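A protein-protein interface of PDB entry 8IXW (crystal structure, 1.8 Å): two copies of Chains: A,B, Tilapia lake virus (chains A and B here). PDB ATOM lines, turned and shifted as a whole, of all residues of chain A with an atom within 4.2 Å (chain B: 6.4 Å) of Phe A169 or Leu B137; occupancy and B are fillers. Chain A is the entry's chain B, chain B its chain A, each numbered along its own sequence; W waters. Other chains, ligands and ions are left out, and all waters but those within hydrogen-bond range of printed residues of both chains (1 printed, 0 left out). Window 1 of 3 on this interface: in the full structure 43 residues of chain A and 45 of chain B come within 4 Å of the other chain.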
ATOM      1  N   CYS A 127      20.423 -15.335  -9.582  1.00  0.00           N
ATOM      2  CA  CYS A 127      20.440 -14.495  -8.389  1.00  0.00           C
ATOM      3  C   CYS A 127      21.265 -13.224  -8.575  1.00  0.00           C
ATOM      4  O   CYS A 127      21.805 -12.689  -7.603  1.00  0.00           O
ATOM      5  CB  CYS A 127      20.947 -15.282  -7.179  1.00  0.00           C
ATOM      6  SG  CYS A 127      22.576 -16.030  -7.376  1.00  0.00           S
ATOM      7  N   ALA A 133      15.197 -14.053  -7.698  1.00  0.00           N
ATOM      8  CA  ALA A 133      15.418 -15.422  -7.244  1.00  0.00           C
ATOM      9  C   ALA A 133      14.346 -15.858  -6.253  1.00  0.00           C
ATOM     10  O   ALA A 133      13.901 -17.010  -6.280  1.00  0.00           O
ATOM     11  CB  ALA A 133      16.807 -15.546  -6.621  1.00  0.00           C
ATOM     12  N   LEU A 134      13.925 -14.957  -5.364  1.00  0.00           N
ATOM     13  CA  LEU A 134      12.878 -15.299  -4.408  1.00  0.00           C
ATOM     14  C   LEU A 134      11.550 -15.550  -5.112  1.00  0.00           C
ATOM     15  O   LEU A 134      10.782 -16.430  -4.706  1.00  0.00           O
ATOM     16  CB  LEU A 134      12.734 -14.188  -3.371  1.00  0.00           C
ATOM     17  CG  LEU A 134      13.889 -14.036  -2.384  1.00  0.00           C
ATOM     18  CD1 LEU A 134      13.690 -12.818  -1.499  1.00  0.00           C
ATOM     19  CD2 LEU A 134      14.023 -15.296  -1.530  1.00  0.00           C
ATOM     20  N   LEU A 137      11.605 -19.078  -6.425  1.00  0.00           N
ATOM     21  CA  LEU A 137      11.378 -20.059  -5.370  1.00  0.00           C
ATOM     22  C   LEU A 137       9.928 -20.043  -4.909  1.00  0.00           C
ATOM     23  O   LEU A 137       9.339 -21.097  -4.642  1.00  0.00           O
ATOM     24  CB  LEU A 137      12.320 -19.798  -4.196  1.00  0.00           C
ATOM     25  CG  LEU A 137      13.802 -20.021  -4.502  1.00  0.00           C
ATOM     26  CD1 LEU A 137      14.677 -19.605  -3.325  1.00  0.00           C
ATOM     27  CD2 LEU A 137      14.065 -21.477  -4.885  1.00  0.00           C
ATOM     28  N   ALA A 165      12.833 -21.155   7.303  1.00  0.00           N
ATOM     29  CA  ALA A 165      13.936 -20.609   6.523  1.00  0.00           C
ATOM     30  C   ALA A 165      13.677 -19.153   6.157  1.00  0.00           C
ATOM     31  O   ALA A 165      14.604 -18.334   6.144  1.00  0.00           O
ATOM     32  CB  ALA A 165      14.155 -21.455   5.271  1.00  0.00           C
ATOM     33  N   ILE A 166      12.425 -18.806   5.862  1.00  0.00           N
ATOM     34  CA  ILE A 166      12.105 -17.416   5.552  1.00  0.00           C
ATOM     35  C   ILE A 166      12.322 -16.534   6.778  1.00  0.00           C
ATOM     36  O   ILE A 166      12.849 -15.421   6.672  1.00  0.00           O
ATOM     37  CB  ILE A 166      10.665 -17.306   5.019  1.00  0.00           C
ATOM     38  CG1 ILE A 166      10.598 -17.842   3.589  1.00  0.00           C
ATOM     39  CG2 ILE A 166      10.186 -15.865   5.072  1.00  0.00           C
ATOM     40  CD1 ILE A 166       9.210 -18.238   3.148  1.00  0.00           C
ATOM     41  N   ASN A 167      11.931 -17.017   7.961  1.00  0.00           N
ATOM     42  CA  ASN A 167      12.141 -16.244   9.183  1.00  0.00           C
ATOM     43  C   ASN A 167      13.625 -16.006   9.439  1.00  0.00           C
ATOM     44  O   ASN A 167      14.025 -14.902   9.830  1.00  0.00           O
ATOM     45  CB  ASN A 167      11.499 -16.959  10.373  1.00  0.00           C
ATOM     46  CG  ASN A 167       9.982 -16.898  10.340  1.00  0.00           C
ATOM     47  OD1 ASN A 167       9.393 -16.263   9.464  1.00  0.00           O
ATOM     48  ND2 ASN A 167       9.342 -17.558  11.297  1.00  0.00           N
ATOM     49  N   HIS A 168      14.459 -17.030   9.235  1.00  0.00           N
ATOM     50  CA  HIS A 168      15.896 -16.842   9.405  1.00  0.00           C
ATOM     51  C   HIS A 168      16.433 -15.839   8.392  1.00  0.00           C
ATOM     52  O   HIS A 168      17.276 -14.995   8.724  1.00  0.00           O
ATOM     53  CB  HIS A 168      16.626 -18.180   9.272  1.00  0.00           C
ATOM     54  CG  HIS A 168      18.078 -18.108   9.622  1.00  0.00           C
ATOM     55  ND1 HIS A 168      19.070 -18.020   8.668  1.00  0.00           N
ATOM     56  CD2 HIS A 168      18.707 -18.093  10.821  1.00  0.00           C
ATOM     57  CE1 HIS A 168      20.248 -17.961   9.267  1.00  0.00           C
ATOM     58  NE2 HIS A 168      20.055 -18.002  10.572  1.00  0.00           N
ATOM     59  N   PHE A 169      15.955 -15.920   7.148  1.00  0.00           N
ATOM     60  CA  PHE A 169      16.340 -14.955   6.119  1.00  0.00           C
ATOM     61  C   PHE A 169      15.965 -13.540   6.539  1.00  0.00           C
ATOM     62  O   PHE A 169      16.785 -12.619   6.463  1.00  0.00           O
ATOM     63  CB  PHE A 169      15.662 -15.336   4.797  1.00  0.00           C
ATOM     64  CG  PHE A 169      16.221 -14.634   3.586  1.00  0.00           C
ATOM     65  CD1 PHE A 169      15.969 -13.292   3.360  1.00  0.00           C
ATOM     66  CD2 PHE A 169      16.981 -15.329   2.662  1.00  0.00           C
ATOM     67  CE1 PHE A 169      16.481 -12.654   2.242  1.00  0.00           C
ATOM     68  CE2 PHE A 169      17.496 -14.698   1.548  1.00  0.00           C
ATOM     69  CZ  PHE A 169      17.246 -13.362   1.336  1.00  0.00           C
ATOM     70  N   ARG A 170      14.724 -13.358   7.004  1.00  0.00           N
ATOM     71  CA  ARG A 170      14.238 -12.042   7.405  1.00  0.00           C
ATOM     72  C   ARG A 170      15.150 -11.387   8.428  1.00  0.00           C
ATOM     73  O   ARG A 170      15.387 -10.174   8.381  1.00  0.00           O
ATOM     74  CB  ARG A 170      12.839 -12.172   8.004  1.00  0.00           C
ATOM     75  CG  ARG A 170      11.733 -12.215   7.003  1.00  0.00           C
ATOM     76  CD  ARG A 170      10.554 -12.976   7.572  1.00  0.00           C
ATOM     77  NE  ARG A 170       9.957 -12.313   8.727  1.00  0.00           N
ATOM     78  CZ  ARG A 170       9.769 -11.003   8.827  1.00  0.00           C
ATOM     79  NH1 ARG A 170      10.134 -10.173   7.864  1.00  0.00           N
ATOM     80  NH2 ARG A 170       9.197 -10.514   9.923  1.00  0.00           N
ATOM     81  N   GLU A 171      15.643 -12.175   9.385  1.00  0.00           N
ATOM     82  CA  GLU A 171      16.464 -11.635  10.461  1.00  0.00           C
ATOM     83  C   GLU A 171      17.641 -10.839   9.926  1.00  0.00           C
ATOM     84  O   GLU A 171      18.077  -9.871  10.558  1.00  0.00           O
ATOM     85  CB  GLU A 171      16.959 -12.778  11.347  1.00  0.00           C
ATOM     86  CG  GLU A 171      15.929 -13.244  12.352  1.00  0.00           C
ATOM     87  CD  GLU A 171      15.630 -12.186  13.391  1.00  0.00           C
ATOM     88  OE1 GLU A 171      16.593 -11.565  13.887  1.00  0.00           O
ATOM     89  OE2 GLU A 171      14.443 -11.976  13.715  1.00  0.00           O
ATOM     90  N   MET A 172      18.167 -11.225   8.765  1.00  0.00           N
ATOM     91  CA  MET A 172      19.297 -10.521   8.182  1.00  0.00           C
ATOM     92  C   MET A 172      18.959  -9.098   7.771  1.00  0.00           C
ATOM     93  O   MET A 172      19.876  -8.314   7.508  1.00  0.00           O
ATOM     94  CB  MET A 172      19.805 -11.279   6.954  1.00  0.00           C
ATOM     95  CG  MET A 172      20.086 -12.751   7.196  1.00  0.00           C
ATOM     96  SD  MET A 172      20.930 -13.527   5.796  1.00  0.00           S
ATOM     97  CE  MET A 172      22.296 -12.392   5.516  1.00  0.00           C
ATOM     98  N   LEU A 173      17.679  -8.750   7.699  1.00  0.00           N
ATOM     99  CA  LEU A 173      17.260  -7.454   7.193  1.00  0.00           C
ATOM    100  C   LEU A 173      16.953  -6.449   8.294  1.00  0.00           C
ATOM    101  O   LEU A 173      16.651  -5.294   7.982  1.00  0.00           O
ATOM    102  CB  LEU A 173      16.030  -7.622   6.295  1.00  0.00           C
ATOM    103  CG  LEU A 173      16.242  -8.435   5.018  1.00  0.00           C
ATOM    104  CD1 LEU A 173      14.903  -8.776   4.382  1.00  0.00           C
ATOM    105  CD2 LEU A 173      17.129  -7.690   4.031  1.00  0.00           C
ATOM    106  N   LYS B  66      26.579 -22.529   1.317  1.00  0.00           N
ATOM    107  CA  LYS B  66      27.196 -21.242   1.624  1.00  0.00           C
ATOM    108  C   LYS B  66      28.686 -21.256   1.293  1.00  0.00           C
ATOM    109  O   LYS B  66      29.211 -20.296   0.723  1.00  0.00           O
ATOM    110  CB  LYS B  66      26.985 -20.880   3.094  1.00  0.00           C
ATOM    111  CG  LYS B  66      25.538 -20.628   3.493  1.00  0.00           C
ATOM    112  CD  LYS B  66      25.401 -20.492   5.004  1.00  0.00           C
ATOM    113  CE  LYS B  66      23.948 -20.298   5.422  1.00  0.00           C
ATOM    114  NZ  LYS B  66      23.400 -19.025   4.882  1.00  0.00           N
ATOM    115  N   THR B 132      17.321 -24.990   1.465  1.00  0.00           N
ATOM    116  CA  THR B 132      18.729 -24.942   1.087  1.00  0.00           C
ATOM    117  C   THR B 132      18.977 -23.827   0.077  1.00  0.00           C
ATOM    118  O   THR B 132      19.996 -23.133   0.148  1.00  0.00           O
ATOM    119  CB  THR B 132      19.174 -26.295   0.530  1.00  0.00           C
ATOM    120  OG1 THR B 132      19.069 -27.292   1.557  1.00  0.00           O
ATOM    121  CG2 THR B 132      20.621 -26.238   0.044  1.00  0.00           C
ATOM    122  N   ALA B 133      18.043 -23.625  -0.856  1.00  0.00           N
ATOM    123  CA  ALA B 133      18.178 -22.516  -1.795  1.00  0.00           C
ATOM    124  C   ALA B 133      18.175 -21.177  -1.066  1.00  0.00           C
ATOM    125  O   ALA B 133      18.936 -20.270  -1.419  1.00  0.00           O
ATOM    126  CB  ALA B 133      17.057 -22.562  -2.834  1.00  0.00           C
ATOM    127  N   LEU B 134      17.323 -21.034  -0.046  1.00  0.00           N
ATOM    128  CA  LEU B 134      17.304 -19.806   0.739  1.00  0.00           C
ATOM    129  C   LEU B 134      18.580 -19.644   1.551  1.00  0.00           C
ATOM    130  O   LEU B 134      19.041 -18.518   1.762  1.00  0.00           O
ATOM    131  CB  LEU B 134      16.091 -19.787   1.668  1.00  0.00           C
ATOM    132  CG  LEU B 134      14.731 -19.589   0.996  1.00  0.00           C
ATOM    133  CD1 LEU B 134      13.589 -20.001   1.918  1.00  0.00           C
ATOM    134  CD2 LEU B 134      14.579 -18.139   0.555  1.00  0.00           C
ATOM    135  N   ALA B 135      19.154 -20.750   2.031  1.00  0.00           N
ATOM    136  CA  ALA B 135      20.442 -20.671   2.711  1.00  0.00           C
ATOM    137  C   ALA B 135      21.513 -20.114   1.782  1.00  0.00           C
ATOM    138  O   ALA B 135      22.363 -19.322   2.201  1.00  0.00           O
ATOM    139  CB  ALA B 135      20.849 -22.053   3.228  1.00  0.00           C
ATOM    140  N   PHE B 136      21.489 -20.520   0.512  1.00  0.00           N
ATOM    141  CA  PHE B 136      22.422 -19.958  -0.456  1.00  0.00           C
ATOM    142  C   PHE B 136      22.134 -18.483  -0.702  1.00  0.00           C
ATOM    143  O   PHE B 136      23.061 -17.666  -0.763  1.00  0.00           O
ATOM    144  CB  PHE B 136      22.353 -20.744  -1.766  1.00  0.00           C
ATOM    145  CG  PHE B 136      23.215 -20.178  -2.858  1.00  0.00           C
ATOM    146  CD1 PHE B 136      24.571 -20.455  -2.909  1.00  0.00           C
ATOM    147  CD2 PHE B 136      22.666 -19.380  -3.847  1.00  0.00           C
ATOM    148  CE1 PHE B 136      25.364 -19.936  -3.919  1.00  0.00           C
ATOM    149  CE2 PHE B 136      23.454 -18.863  -4.856  1.00  0.00           C
ATOM    150  CZ  PHE B 136      24.801 -19.142  -4.893  1.00  0.00           C
ATOM    151  N   LEU B 137      20.856 -18.122  -0.845  1.00  0.00           N
ATOM    152  CA  LEU B 137      20.509 -16.732  -1.123  1.00  0.00           C
ATOM    153  C   LEU B 137      20.848 -15.829   0.059  1.00  0.00           C
ATOM    154  O   LEU B 137      21.109 -14.636  -0.134  1.00  0.00           O
ATOM    155  CB  LEU B 137      19.027 -16.621  -1.478  1.00  0.00           C
ATOM    156  CG  LEU B 137      18.621 -17.078  -2.883  1.00  0.00           C
ATOM    157  CD1 LEU B 137      17.113 -16.927  -3.101  1.00  0.00           C
ATOM    158  CD2 LEU B 137      19.382 -16.319  -3.957  1.00  0.00           C
ATOM    159  N   GLU B 138      20.854 -16.373   1.279  1.00  0.00           N
ATOM    160  CA  GLU B 138      21.330 -15.607   2.426  1.00  0.00           C
ATOM    161  C   GLU B 138      22.777 -15.175   2.232  1.00  0.00           C
ATOM    162  O   GLU B 138      23.159 -14.058   2.600  1.00  0.00           O
ATOM    163  CB  GLU B 138      21.214 -16.432   3.708  1.00  0.00           C
ATOM    164  CG  GLU B 138      19.821 -16.536   4.260  1.00  0.00           C
ATOM    165  CD  GLU B 138      19.758 -17.398   5.495  1.00  0.00           C
ATOM    166  OE1 GLU B 138      20.796 -17.989   5.873  1.00  0.00           O
ATOM    167  OE2 GLU B 138      18.663 -17.486   6.085  1.00  0.00           O
ATOM    168  N   GLU B 139      23.604 -16.067   1.679  1.00  0.00           N
ATOM    169  CA  GLU B 139      24.995 -15.725   1.407  1.00  0.00           C
ATOM    170  C   GLU B 139      25.095 -14.668   0.315  1.00  0.00           C
ATOM    171  O   GLU B 139      25.927 -13.756   0.402  1.00  0.00           O
ATOM    172  CB  GLU B 139      25.767 -16.985   1.018  1.00  0.00           C
ATOM    173  CG  GLU B 139      27.270 -16.795   0.938  1.00  0.00           C
ATOM    174  CD  GLU B 139      27.929 -16.665   2.299  1.00  0.00           C
ATOM    175  OE1 GLU B 139      27.278 -16.974   3.323  1.00  0.00           O
ATOM    176  OE2 GLU B 139      29.103 -16.246   2.340  1.00  0.00           O
ATOM    177  N   VAL B 140      24.260 -14.769  -0.720  1.00  0.00           N
ATOM    178  CA  VAL B 140      24.225 -13.729  -1.744  1.00  0.00           C
ATOM    179  C   VAL B 140      23.885 -12.387  -1.108  1.00  0.00           C
ATOM    180  O   VAL B 140      24.540 -11.369  -1.368  1.00  0.00           O
ATOM    181  CB  VAL B 140      23.223 -14.096  -2.852  1.00  0.00           C
ATOM    182  CG1 VAL B 140      23.114 -12.968  -3.881  1.00  0.00           C
ATOM    183  CG2 VAL B 140      23.614 -15.404  -3.526  1.00  0.00           C
ATOM    184  N   LEU B 141      22.859 -12.372  -0.252  1.00  0.00           N
ATOM    185  CA  LEU B 141      22.438 -11.132   0.394  1.00  0.00           C
ATOM    186  C   LEU B 141      23.546 -10.565   1.272  1.00  0.00           C
ATOM    187  O   LEU B 141      23.871  -9.376   1.189  1.00  0.00           O
ATOM    188  CB  LEU B 141      21.169 -11.376   1.215  1.00  0.00           C
ATOM    189  CG  LEU B 141      20.714 -10.221   2.108  1.00  0.00           C
ATOM    190  CD1 LEU B 141      20.337  -9.016   1.259  1.00  0.00           C
ATOM    191  CD2 LEU B 141      19.549 -10.636   3.001  1.00  0.00           C
ATOM    192  N   ALA B 142      24.140 -11.405   2.123  1.00  0.00           N
ATOM    193  CA  ALA B 142      25.198 -10.933   3.013  1.00  0.00           C
ATOM    194  C   ALA B 142      26.361 -10.353   2.223  1.00  0.00           C
ATOM    195  O   ALA B 142      26.932  -9.325   2.605  1.00  0.00           O
ATOM    196  CB  ALA B 142      25.679 -12.073   3.911  1.00  0.00           C
ATOM    197  N   THR B 162      14.647  -6.487  -1.053  1.00  0.00           N
ATOM    198  CA  THR B 162      14.635  -7.862  -0.571  1.00  0.00           C
ATOM    199  C   THR B 162      13.532  -8.069   0.459  1.00  0.00           C
ATOM    200  O   THR B 162      12.846  -9.096   0.444  1.00  0.00           O
ATOM    201  CB  THR B 162      15.998  -8.220   0.012  1.00  0.00           C
ATOM    202  OG1 THR B 162      17.004  -7.995  -0.983  1.00  0.00           O
ATOM    203  CG2 THR B 162      16.025  -9.674   0.445  1.00  0.00           C
ATOM    204  N   ILE B 166      10.664 -10.900   0.329  1.00  0.00           N
ATOM    205  CA  ILE B 166      10.542 -11.937   1.350  1.00  0.00           C
ATOM    206  C   ILE B 166       9.175 -11.854   2.023  1.00  0.00           C
ATOM    207  O   ILE B 166       8.605 -12.882   2.406  1.00  0.00           O
ATOM    208  CB  ILE B 166      11.719 -11.830   2.337  1.00  0.00           C
ATOM    209  CG1 ILE B 166      11.978 -13.170   3.042  1.00  0.00           C
ATOM    210  CG2 ILE B 166      11.470 -10.764   3.384  1.00  0.00           C
ATOM    211  CD1 ILE B 166      12.385 -14.298   2.107  1.00  0.00           C
HETATM  212  O   HOH W   1      16.912 -19.169   4.930  1.00  0.00           O
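N of Phe A169 is in hydrogen-bond range of OE2 of Glu B138, 3.3 Å away. A ring nitrogen (ND1) of His A168 is in hydrogen-bond range of the side-chain carboxylate of Glu B138 (2.7 Å).
The side-chain amino group (NZ) of Lys B66 is in salt-bridge range of the side-chain carboxylate (OE1) of Glu B138, 3.0 Å away.
Among the printed residues, merely in contact across the chains: Cys A127 with Phe B136, Cys A127 with Leu B137, Cys A127 with Val B140, Ala A133 with Leu B137, Leu A134 with Leu B134, Leu A134 with Leu B137, Leu A137 with Ala B133, Leu A137 with Leu B137, Ala A165 with Leu B134, Ile A166 with Ile B166, Phe A169 with Leu B134, Phe A169 with Leu B137, Phe A169 with Leu B141, Phe A169 with Thr B162, Phe A169 with Ile B166, Arg A170 with Ile B166, Met A172 with Glu B138, Met A172 with Ala B142 and Leu A173 with Leu B141.
Of the printed residues of chain B, Ile A166 touches Ile B166 (3.8 Å). Of the printed residues of chain B, His A168 touches Glu B138. Printed residues of chain B within 4 Å of Phe A169: Leu B134, Leu B137, Glu B138, Leu B141, Thr B162 and Ile B166. Of the printed residues of chain A, Ala B133 touches Leu A137. Leu B137 touches five residues of chain A. The nearest printed residue of chain A that does not touch Leu B137 is Met A172 (6.0 Å). The nearest printed residue of chain B that does not touch Arg A170 is Glu B138 (5.8 Å).
Along chain A the printed residues that touch a printed residue of chain B span positions 127 to 173. Of the 14 printed residues of chain B, 10 touch a printed residue of chain A. Printed residues of chain B that touch a printed residue of chain A: Ala B133, Leu B134, Phe B136, Leu B137, Glu B138, Val B140, Leu B141, Ala B142, Thr B162 and Ile B166. Hydrophobic or aromatic side chains of chain B within 4 Å of the printed part of chain A: Ala B133, Leu B134, Phe B136, Leu B137, Val B140, Leu B141, Ala B142 and Ile B166. Along chain B the printed residues that touch a printed residue of chain A span positions 133 to 166. Among the printed residues, 21 pairs touch across the chains. Among the printed residues, no Asp or Glu carboxylate lies within 4 Å of a Lys or Arg side-chain nitrogen of the other chain.
Leu A134 touches its own counterpart, Leu B134. Leu A134 touches Leu B137, but with the chains exchanged Leu A137 does not touch Leu B134 (4.1 Å). Leu A137 touches its own counterpart, Leu B137. Ile B166 touches its own counterpart, Ile A166. 4 positions are printed for both chains.
Water W1 lies within hydrogen-bond range of OE2 of Glu B138 (2.7 Å) and O of Ala A165 (2.7 Å).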
